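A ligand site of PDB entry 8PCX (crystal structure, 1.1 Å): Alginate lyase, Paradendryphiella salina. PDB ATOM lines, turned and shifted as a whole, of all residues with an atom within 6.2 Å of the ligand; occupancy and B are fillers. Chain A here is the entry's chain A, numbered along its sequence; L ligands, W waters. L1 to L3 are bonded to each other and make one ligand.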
ATOM      1  N   SER A  60      -2.204 -38.684  -5.630  1.00  0.00           N
ATOM      2  CA  SER A  60      -1.790 -37.672  -4.655  1.00  0.00           C
ATOM      3  C   SER A  60      -0.319 -37.774  -4.288  1.00  0.00           C
ATOM      4  O   SER A  60       0.150 -37.000  -3.440  1.00  0.00           O
ATOM      5  CB  SER A  60      -2.689 -37.575  -3.416  1.00  0.00           C
ATOM      6  OG  SER A  60      -2.394 -38.583  -2.466  1.00  0.00           O
ATOM      7  N   GLU A 103      -4.230 -35.804 -14.569  1.00  0.00           N
ATOM      8  CA  GLU A 103      -3.929 -34.421 -14.220  1.00  0.00           C
ATOM      9  C   GLU A 103      -2.595 -34.431 -13.492  1.00  0.00           C
ATOM     10  O   GLU A 103      -2.396 -35.242 -12.593  1.00  0.00           O
ATOM     11  CB  GLU A 103      -5.004 -33.803 -13.327  1.00  0.00           C
ATOM     12  CG  GLU A 103      -4.624 -32.397 -12.859  1.00  0.00           C
ATOM     13  CD  GLU A 103      -5.708 -31.654 -12.092  1.00  0.00           C
ATOM     14  OE1 GLU A 103      -6.663 -32.303 -11.603  1.00  0.00           O
ATOM     15  OE2 GLU A 103      -5.603 -30.402 -11.970  1.00  0.00           O
ATOM     16  N   THR A 105      -0.089 -31.627 -11.622  1.00  0.00           N
ATOM     17  CA  THR A 105       0.223 -30.276 -11.180  1.00  0.00           C
ATOM     18  C   THR A 105       1.731 -30.056 -11.296  1.00  0.00           C
ATOM     19  O   THR A 105       2.528 -30.849 -10.801  1.00  0.00           O
ATOM     20  CB  THR A 105      -0.262 -30.090  -9.738  1.00  0.00           C
ATOM     21  OG1 THR A 105      -1.683 -30.166  -9.697  1.00  0.00           O
ATOM     22  CG2 THR A 105       0.194 -28.757  -9.159  1.00  0.00           C
ATOM     23  N   GLN A 108       2.856 -24.637  -8.199  1.00  0.00           N
ATOM     24  CA  GLN A 108       1.862 -24.257  -7.197  1.00  0.00           C
ATOM     25  C   GLN A 108       2.279 -23.000  -6.455  1.00  0.00           C
ATOM     26  O   GLN A 108       3.467 -22.671  -6.327  1.00  0.00           O
ATOM     27  CB  GLN A 108       1.665 -25.329  -6.122  1.00  0.00           C
ATOM     28  CG  GLN A 108       1.361 -26.698  -6.648  1.00  0.00           C
ATOM     29  CD  GLN A 108       0.748 -27.594  -5.584  1.00  0.00           C
ATOM     30  OE1 GLN A 108      -0.267 -27.223  -4.978  1.00  0.00           O
ATOM     31  NE2 GLN A 108       1.335 -28.762  -5.347  1.00  0.00           N
ATOM     32  N   HIS A 110       1.165 -22.657  -2.553  1.00  0.00           N
ATOM     33  CA  HIS A 110       0.494 -23.441  -1.515  1.00  0.00           C
ATOM     34  C   HIS A 110       0.784 -22.802  -0.173  1.00  0.00           C
ATOM     35  O   HIS A 110       1.778 -22.088  -0.019  1.00  0.00           O
ATOM     36  CB  HIS A 110       1.006 -24.914  -1.525  1.00  0.00           C
ATOM     37  CG  HIS A 110       0.010 -25.923  -1.033  1.00  0.00           C
ATOM     38  ND1 HIS A 110      -0.265 -26.133   0.302  1.00  0.00           N
ATOM     39  CD2 HIS A 110      -0.756 -26.803  -1.717  1.00  0.00           C
ATOM     40  CE1 HIS A 110      -1.183 -27.076   0.416  1.00  0.00           C
ATOM     41  NE2 HIS A 110      -1.490 -27.511  -0.793  1.00  0.00           N
ATOM     42  N   PRO A 115      -4.017 -25.092  -1.450  1.00  0.00           N
ATOM     43  CA  PRO A 115      -3.389 -24.549  -2.660  1.00  0.00           C
ATOM     44  C   PRO A 115      -4.063 -23.272  -3.130  1.00  0.00           C
ATOM     45  O   PRO A 115      -5.211 -23.288  -3.594  1.00  0.00           O
ATOM     46  CB  PRO A 115      -3.611 -25.670  -3.670  1.00  0.00           C
ATOM     47  CG  PRO A 115      -4.924 -26.291  -3.209  1.00  0.00           C
ATOM     48  CD  PRO A 115      -4.973 -26.180  -1.736  1.00  0.00           C
ATOM     49  N   ARG A 118      -2.805 -23.902  -8.478  1.00  0.00           N
ATOM     50  CA  ARG A 118      -2.147 -25.016  -9.153  1.00  0.00           C
ATOM     51  C   ARG A 118      -2.183 -24.752 -10.651  1.00  0.00           C
ATOM     52  O   ARG A 118      -3.249 -24.492 -11.216  1.00  0.00           O
ATOM     53  CB  ARG A 118      -2.837 -26.350  -8.878  1.00  0.00           C
ATOM     54  CG  ARG A 118      -2.817 -26.746  -7.414  1.00  0.00           C
ATOM     55  CD  ARG A 118      -3.390 -28.126  -7.155  1.00  0.00           C
ATOM     56  NE  ARG A 118      -4.783 -28.208  -7.550  1.00  0.00           N
ATOM     57  CZ  ARG A 118      -5.236 -28.737  -8.673  1.00  0.00           C
ATOM     58  NH1 ARG A 118      -4.430 -29.342  -9.535  1.00  0.00           N
ATOM     59  NH2 ARG A 118      -6.545 -28.669  -8.936  1.00  0.00           N
ATOM     60  N   LYS A 125     -11.225 -31.941 -19.893  1.00  0.00           N
ATOM     61  CA  LYS A 125     -12.107 -31.274 -18.941  1.00  0.00           C
ATOM     62  C   LYS A 125     -12.884 -30.195 -19.655  1.00  0.00           C
ATOM     63  O   LYS A 125     -12.380 -29.565 -20.590  1.00  0.00           O
ATOM     64  CB  LYS A 125     -11.296 -30.639 -17.799  1.00  0.00           C
ATOM     65  CG  LYS A 125     -12.192 -30.094 -16.687  1.00  0.00           C
ATOM     66  CD  LYS A 125     -11.430 -29.738 -15.425  1.00  0.00           C
ATOM     67  CE  LYS A 125     -10.830 -30.963 -14.718  1.00  0.00           C
ATOM     68  NZ  LYS A 125     -11.819 -31.736 -13.917  1.00  0.00           N
ATOM     69  N   SER A 126     -14.114 -29.963 -19.191  1.00  0.00           N
ATOM     70  CA  SER A 126     -14.901 -28.835 -19.651  1.00  0.00           C
ATOM     71  C   SER A 126     -14.844 -27.687 -18.662  1.00  0.00           C
ATOM     72  O   SER A 126     -14.946 -27.897 -17.450  1.00  0.00           O
ATOM     73  CB  SER A 126     -16.343 -29.259 -19.890  1.00  0.00           C
ATOM     74  OG  SER A 126     -16.402 -30.135 -20.999  1.00  0.00           O
ATOM     75  N   LEU A 127     -14.647 -26.479 -19.170  1.00  0.00           N
ATOM     76  CA  LEU A 127     -14.594 -25.267 -18.376  1.00  0.00           C
ATOM     77  C   LEU A 127     -15.536 -24.253 -18.990  1.00  0.00           C
ATOM     78  O   LEU A 127     -15.417 -23.935 -20.185  1.00  0.00           O
ATOM     79  CB  LEU A 127     -13.194 -24.666 -18.371  1.00  0.00           C
ATOM     80  CG  LEU A 127     -12.090 -25.557 -17.811  1.00  0.00           C
ATOM     81  CD1 LEU A 127     -10.742 -24.887 -17.950  1.00  0.00           C
ATOM     82  CD2 LEU A 127     -12.356 -25.893 -16.350  1.00  0.00           C
ATOM     83  N   MET A 137      -3.887 -25.810 -17.410  1.00  0.00           N
ATOM     84  CA  MET A 137      -4.940 -25.106 -16.713  1.00  0.00           C
ATOM     85  C   MET A 137      -4.401 -24.434 -15.452  1.00  0.00           C
ATOM     86  O   MET A 137      -3.428 -24.894 -14.868  1.00  0.00           O
ATOM     87  CB  MET A 137      -5.982 -26.157 -16.276  1.00  0.00           C
ATOM     88  CG  MET A 137      -7.271 -25.614 -15.704  1.00  0.00           C
ATOM     89  SD  MET A 137      -8.519 -26.898 -15.506  1.00  0.00           S
ATOM     90  CE  MET A 137      -7.863 -27.817 -14.148  1.00  0.00           C
ATOM     91  N   THR A 139      -5.860 -23.416 -11.632  1.00  0.00           N
ATOM     92  CA  THR A 139      -6.923 -23.560 -10.647  1.00  0.00           C
ATOM     93  C   THR A 139      -6.540 -22.682  -9.467  1.00  0.00           C
ATOM     94  O   THR A 139      -5.558 -22.950  -8.779  1.00  0.00           O
ATOM     95  CB  THR A 139      -7.093 -25.011 -10.190  1.00  0.00           C
ATOM     96  OG1 THR A 139      -7.402 -25.840 -11.321  1.00  0.00           O
ATOM     97  CG2 THR A 139      -8.222 -25.132  -9.175  1.00  0.00           C
ATOM     98  N   ARG A 141      -7.822 -21.003  -5.851  1.00  0.00           N
ATOM     99  CA  ARG A 141      -8.798 -21.008  -4.770  1.00  0.00           C
ATOM    100  C   ARG A 141      -9.066 -19.597  -4.289  1.00  0.00           C
ATOM    101  O   ARG A 141      -8.134 -18.861  -3.946  1.00  0.00           O
ATOM    102  CB  ARG A 141      -8.352 -21.870  -3.583  1.00  0.00           C
ATOM    103  CG  ARG A 141      -8.754 -23.318  -3.704  1.00  0.00           C
ATOM    104  CD  ARG A 141      -8.404 -24.060  -2.426  1.00  0.00           C
ATOM    105  NE  ARG A 141      -8.930 -25.423  -2.383  1.00  0.00           N
ATOM    106  CZ  ARG A 141     -10.167 -25.751  -2.035  1.00  0.00           C
ATOM    107  NH1 ARG A 141     -11.061 -24.847  -1.677  1.00  0.00           N
ATOM    108  NH2 ARG A 141     -10.514 -27.035  -2.043  1.00  0.00           N
ATOM    109  N   ASP A 146     -15.785 -26.604  -1.007  1.00  0.00           N
ATOM    110  CA  ASP A 146     -15.697 -27.596  -2.065  1.00  0.00           C
ATOM    111  C   ASP A 146     -16.531 -27.233  -3.288  1.00  0.00           C
ATOM    112  O   ASP A 146     -16.312 -27.813  -4.357  1.00  0.00           O
ATOM    113  CB  ASP A 146     -16.169 -28.962  -1.550  1.00  0.00           C
ATOM    114  CG  ASP A 146     -17.602 -28.928  -1.027  1.00  0.00           C
ATOM    115  OD1 ASP A 146     -17.842 -28.411   0.089  1.00  0.00           O
ATOM    116  OD2 ASP A 146     -18.509 -29.417  -1.737  1.00  0.00           O
ATOM    117  N   SER A 148     -18.074 -25.178  -6.536  1.00  0.00           N
ATOM    118  CA  SER A 148     -17.341 -24.577  -7.645  1.00  0.00           C
ATOM    119  C   SER A 148     -17.103 -23.085  -7.451  1.00  0.00           C
ATOM    120  O   SER A 148     -16.179 -22.541  -8.055  1.00  0.00           O
ATOM    121  CB  SER A 148     -18.070 -24.829  -8.958  1.00  0.00           C
ATOM    122  OG  SER A 148     -19.375 -24.271  -8.913  1.00  0.00           O
ATOM    123  N   PHE A 151     -13.469 -21.792  -6.603  1.00  0.00           N
ATOM    124  CA  PHE A 151     -12.381 -21.964  -7.542  1.00  0.00           C
ATOM    125  C   PHE A 151     -12.585 -21.084  -8.754  1.00  0.00           C
ATOM    126  O   PHE A 151     -13.721 -20.832  -9.170  1.00  0.00           O
ATOM    127  CB  PHE A 151     -12.299 -23.415  -8.037  1.00  0.00           C
ATOM    128  CG  PHE A 151     -12.204 -24.421  -6.946  1.00  0.00           C
ATOM    129  CD1 PHE A 151     -10.982 -24.802  -6.432  1.00  0.00           C
ATOM    130  CD2 PHE A 151     -13.346 -24.977  -6.410  1.00  0.00           C
ATOM    131  CE1 PHE A 151     -10.898 -25.722  -5.412  1.00  0.00           C
ATOM    132  CE2 PHE A 151     -13.268 -25.894  -5.383  1.00  0.00           C
ATOM    133  CZ  PHE A 151     -12.050 -26.276  -4.886  1.00  0.00           C
ATOM    134  N   LYS A 153     -11.100 -21.568 -12.503  1.00  0.00           N
ATOM    135  CA  LYS A 153     -10.359 -22.499 -13.341  1.00  0.00           C
ATOM    136  C   LYS A 153     -10.311 -21.981 -14.776  1.00  0.00           C
ATOM    137  O   LYS A 153     -11.372 -21.740 -15.371  1.00  0.00           O
ATOM    138  CB  LYS A 153     -11.017 -23.878 -13.342  1.00  0.00           C
ATOM    139  CG  LYS A 153     -10.936 -24.610 -12.004  1.00  0.00           C
ATOM    140  CD  LYS A 153     -11.421 -26.055 -12.132  1.00  0.00           C
ATOM    141  CE  LYS A 153     -11.103 -26.881 -10.920  1.00  0.00           C
ATOM    142  NZ  LYS A 153     -11.884 -28.148 -10.936  1.00  0.00           N
ATOM    143  N   TYR A 206       3.001 -33.447  -9.459  1.00  0.00           N
ATOM    144  CA  TYR A 206       2.098 -33.842  -8.387  1.00  0.00           C
ATOM    145  C   TYR A 206       0.867 -34.433  -9.057  1.00  0.00           C
ATOM    146  O   TYR A 206       0.196 -33.752  -9.845  1.00  0.00           O
ATOM    147  CB  TYR A 206       1.805 -32.616  -7.506  1.00  0.00           C
ATOM    148  CG  TYR A 206       0.677 -32.732  -6.521  1.00  0.00           C
ATOM    149  CD1 TYR A 206       0.444 -33.882  -5.772  1.00  0.00           C
ATOM    150  CD2 TYR A 206      -0.148 -31.648  -6.324  1.00  0.00           C
ATOM    151  CE1 TYR A 206      -0.593 -33.936  -4.854  1.00  0.00           C
ATOM    152  CE2 TYR A 206      -1.178 -31.692  -5.432  1.00  0.00           C
ATOM    153  CZ  TYR A 206      -1.400 -32.840  -4.703  1.00  0.00           C
ATOM    154  OH  TYR A 206      -2.437 -32.882  -3.803  1.00  0.00           O
ATOM    155  N   ASN A 208      -2.642 -36.014  -9.780  1.00  0.00           N
ATOM    156  CA  ASN A 208      -3.984 -35.815  -9.250  1.00  0.00           C
ATOM    157  C   ASN A 208      -4.988 -36.712  -9.963  1.00  0.00           C
ATOM    158  O   ASN A 208      -5.058 -36.717 -11.192  1.00  0.00           O
ATOM    159  CB  ASN A 208      -4.410 -34.350  -9.440  1.00  0.00           C
ATOM    160  CG  ASN A 208      -3.330 -33.359  -9.047  1.00  0.00           C
ATOM    161  OD1 ASN A 208      -2.907 -32.551  -9.871  1.00  0.00           O
ATOM    162  ND2 ASN A 208      -2.883 -33.412  -7.804  1.00  0.00           N
ATOM    163  N   ASN A 209      -5.775 -37.454  -9.186  1.00  0.00           N
ATOM    164  CA  ASN A 209      -6.869 -38.260  -9.706  1.00  0.00           C
ATOM    165  C   ASN A 209      -6.516 -39.169 -10.892  1.00  0.00           C
ATOM    166  O   ASN A 209      -7.243 -39.212 -11.875  1.00  0.00           O
ATOM    167  CB  ASN A 209      -8.040 -37.368 -10.088  1.00  0.00           C
ATOM    168  CG  ASN A 209      -8.574 -36.568  -8.927  1.00  0.00           C
ATOM    169  OD1 ASN A 209      -8.679 -37.069  -7.818  1.00  0.00           O
ATOM    170  ND2 ASN A 209      -8.904 -35.312  -9.189  1.00  0.00           N
HETATM  171  C1  LIG L   1      -5.122 -31.177  -3.964  1.00  0.00           C
HETATM  172  O1  LIG L   1      -4.315 -30.382  -4.588  1.00  0.00           O
HETATM  173  C2  LIG L   1      -5.768 -32.150  -4.982  1.00  0.00           C
HETATM  174  O2  LIG L   1      -6.618 -33.034  -4.265  1.00  0.00           O
HETATM  175  C3  LIG L   1      -6.554 -31.428  -6.031  1.00  0.00           C
HETATM  176  O3  LIG L   1      -7.127 -32.420  -6.933  1.00  0.00           O
HETATM  177  C4  LIG L   1      -7.576 -30.562  -5.410  1.00  0.00           C
HETATM  178  O4  LIG L   1      -8.170 -29.774  -6.465  1.00  0.00           O
HETATM  179  C5  LIG L   1      -6.958 -29.607  -4.440  1.00  0.00           C
HETATM  180  O5  LIG L   1      -6.286 -30.382  -3.390  1.00  0.00           O
HETATM  181  C6  LIG L   1      -7.969 -28.723  -3.745  1.00  0.00           C
HETATM  182  O6  LIG L   1      -8.054 -27.531  -4.096  1.00  0.00           O
HETATM  183  O7  LIG L   1      -8.675 -29.216  -2.822  1.00  0.00           O
HETATM  184  C1  LG2 L   2      -9.576 -29.809  -6.410  1.00  0.00           C
HETATM  185  C2  LG2 L   2     -10.173 -28.819  -7.376  1.00  0.00           C
HETATM  186  O1  LG2 L   2      -9.615 -29.016  -8.690  1.00  0.00           O
HETATM  187  C3  LG2 L   2     -11.664 -29.030  -7.346  1.00  0.00           C
HETATM  188  O2  LG2 L   2     -12.231 -28.092  -8.292  1.00  0.00           O
HETATM  189  C4  LG2 L   2     -12.022 -30.476  -7.611  1.00  0.00           C
HETATM  190  O3  LG2 L   2     -13.415 -30.726  -7.435  1.00  0.00           O
HETATM  191  C5  LG2 L   2     -11.328 -31.404  -6.608  1.00  0.00           C
HETATM  192  O4  LG2 L   2      -9.895 -31.213  -6.726  1.00  0.00           O
HETATM  193  C6  LG2 L   2     -11.498 -32.878  -6.775  1.00  0.00           C
HETATM  194  O5  LG2 L   2     -11.469 -33.630  -5.744  1.00  0.00           O
HETATM  195  O6  LG2 L   2     -11.600 -33.371  -7.917  1.00  0.00           O
HETATM  196  C1  LG3 L   3     -13.944 -31.334  -8.611  1.00  0.00           C
HETATM  197  C2  LG3 L   3     -15.304 -31.942  -8.324  1.00  0.00           C
HETATM  198  O1  LG3 L   3     -16.213 -30.882  -7.956  1.00  0.00           O
HETATM  199  C3  LG3 L   3     -15.770 -32.670  -9.539  1.00  0.00           C
HETATM  200  O2  LG3 L   3     -17.037 -33.345  -9.269  1.00  0.00           O
HETATM  201  C4  LG3 L   3     -15.856 -31.719 -10.713  1.00  0.00           C
HETATM  202  O3  LG3 L   3     -16.240 -32.468 -11.873  1.00  0.00           O
HETATM  203  C5  LG3 L   3     -14.501 -31.038 -10.948  1.00  0.00           C
HETATM  204  O4  LG3 L   3     -14.047 -30.350  -9.729  1.00  0.00           O
HETATM  205  C6  LG3 L   3     -14.532 -30.022 -12.040  1.00  0.00           C
HETATM  206  O5  LG3 L   3     -14.281 -30.378 -13.223  1.00  0.00           O
HETATM  207  O6  LG3 L   3     -14.791 -28.820 -11.767  1.00  0.00           O
HETATM  208  O   HOH W   1     -10.680 -32.515 -10.416  1.00  0.00           O
HETATM  209  O   HOH W   2     -14.602 -26.647  -9.587  1.00  0.00           O
HETATM  210  O   HOH W   3      -8.537 -34.591  -5.797  1.00  0.00           O
HETATM  211  O   HOH W   4      -8.132 -31.529  -9.287  1.00  0.00           O
HETATM  212  O   HOH W   5     -11.241 -30.149  -2.989  1.00  0.00           O
HETATM  213  O   HOH W   6     -14.260 -30.081  -4.233  1.00  0.00           O
HETATM  214  O   HOH W   7     -15.104 -28.557  -7.611  1.00  0.00           O
HETATM  215  O   HOH W   8      -6.856 -26.727  -6.378  1.00  0.00           O
HETATM  216  O   HOH W   9     -18.389 -30.120  -8.656  1.00  0.00           O
HETATM  217  O   HOH W  10      -3.178 -29.565  -2.009  1.00  0.00           O
HETATM  218  O   HOH W  11     -13.397 -35.469  -5.728  1.00  0.00           O
HETATM  219  O   HOH W  12      -5.191 -34.630  -2.451  1.00  0.00           O
HETATM  220  O   HOH W  13     -19.120 -34.351 -10.556  1.00  0.00           O
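The side-chain hydroxyl of Tyr 206 sits close to an oxygen (O1) of LIG L1 (3.2 Å).
The guanidinium group (NH2) of Arg 118 is in hydrogen-bond range of an oxygen (O1) of LG2 L2 (3.1 Å).
NZ of Lys 153 is in salt-bridge range of O6 of LG3 L3 (3.1 Å).
NZ of Lys 125 lies within salt-bridge range of O5 of LG3 L3, 2.9 Å away.
NE of Arg 141 lies within salt-bridge range of O6 of LIG L1.
The guanidinium group of Arg 118 lies within hydrogen-bond range of the side-chain hydroxyl of Thr 105.
The backbone carbonyl oxygen of Arg 118 is in hydrogen-bond range of the backbone NH of Thr 139 (2.9 Å).
The backbone carbonyl oxygen of Tyr 206 is in hydrogen-bond range of the backbone NH of Thr 105.
The side-chain carboxylate (OE2) of Glu 103 lies within salt-bridge range of the guanidinium group (NH1) of Arg 118, at 2.9 Å.
The backbone carbonyl oxygen of Tyr 206 lies close to the side-chain amide oxygen of Asn 208 (3.3 Å).
Merely in contact with the ligand: Pro 115 (3.5 Å), Asn 209 (3.6 Å) and Phe 151 (3.6 Å).
Hydrophobic or aromatic side chains that line the ligand: Pro 115, Phe 151 and Tyr 206.
Water W8 bridges O6 of LIG L1 (2.7 Å) and NE of Arg 118 (2.8 Å).
Water W4 lies within hydrogen-bond range of an oxygen (O3) of LIG L1, the side-chain carboxylate (OE1) of Glu 103 and the guanidinium group (NH2) of Arg 118.
Water W3 lies within hydrogen-bond range of O3 of LIG L1 (2.8 Å) and OD1 of Asn 209 (3.2 Å).
Water W10 lies within hydrogen-bond range of NE2 of His 110 (2.9 Å) and O1 of LIG L1 (2.9 Å).
Water W2 bridges an oxygen (O2) of LG2 L2 and the side-chain amino group of Lys 153.
Water W6 lies within hydrogen-bond range of the backbone carbonyl oxygen of Asp 146 and an oxygen (O3) of LG2 L2.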
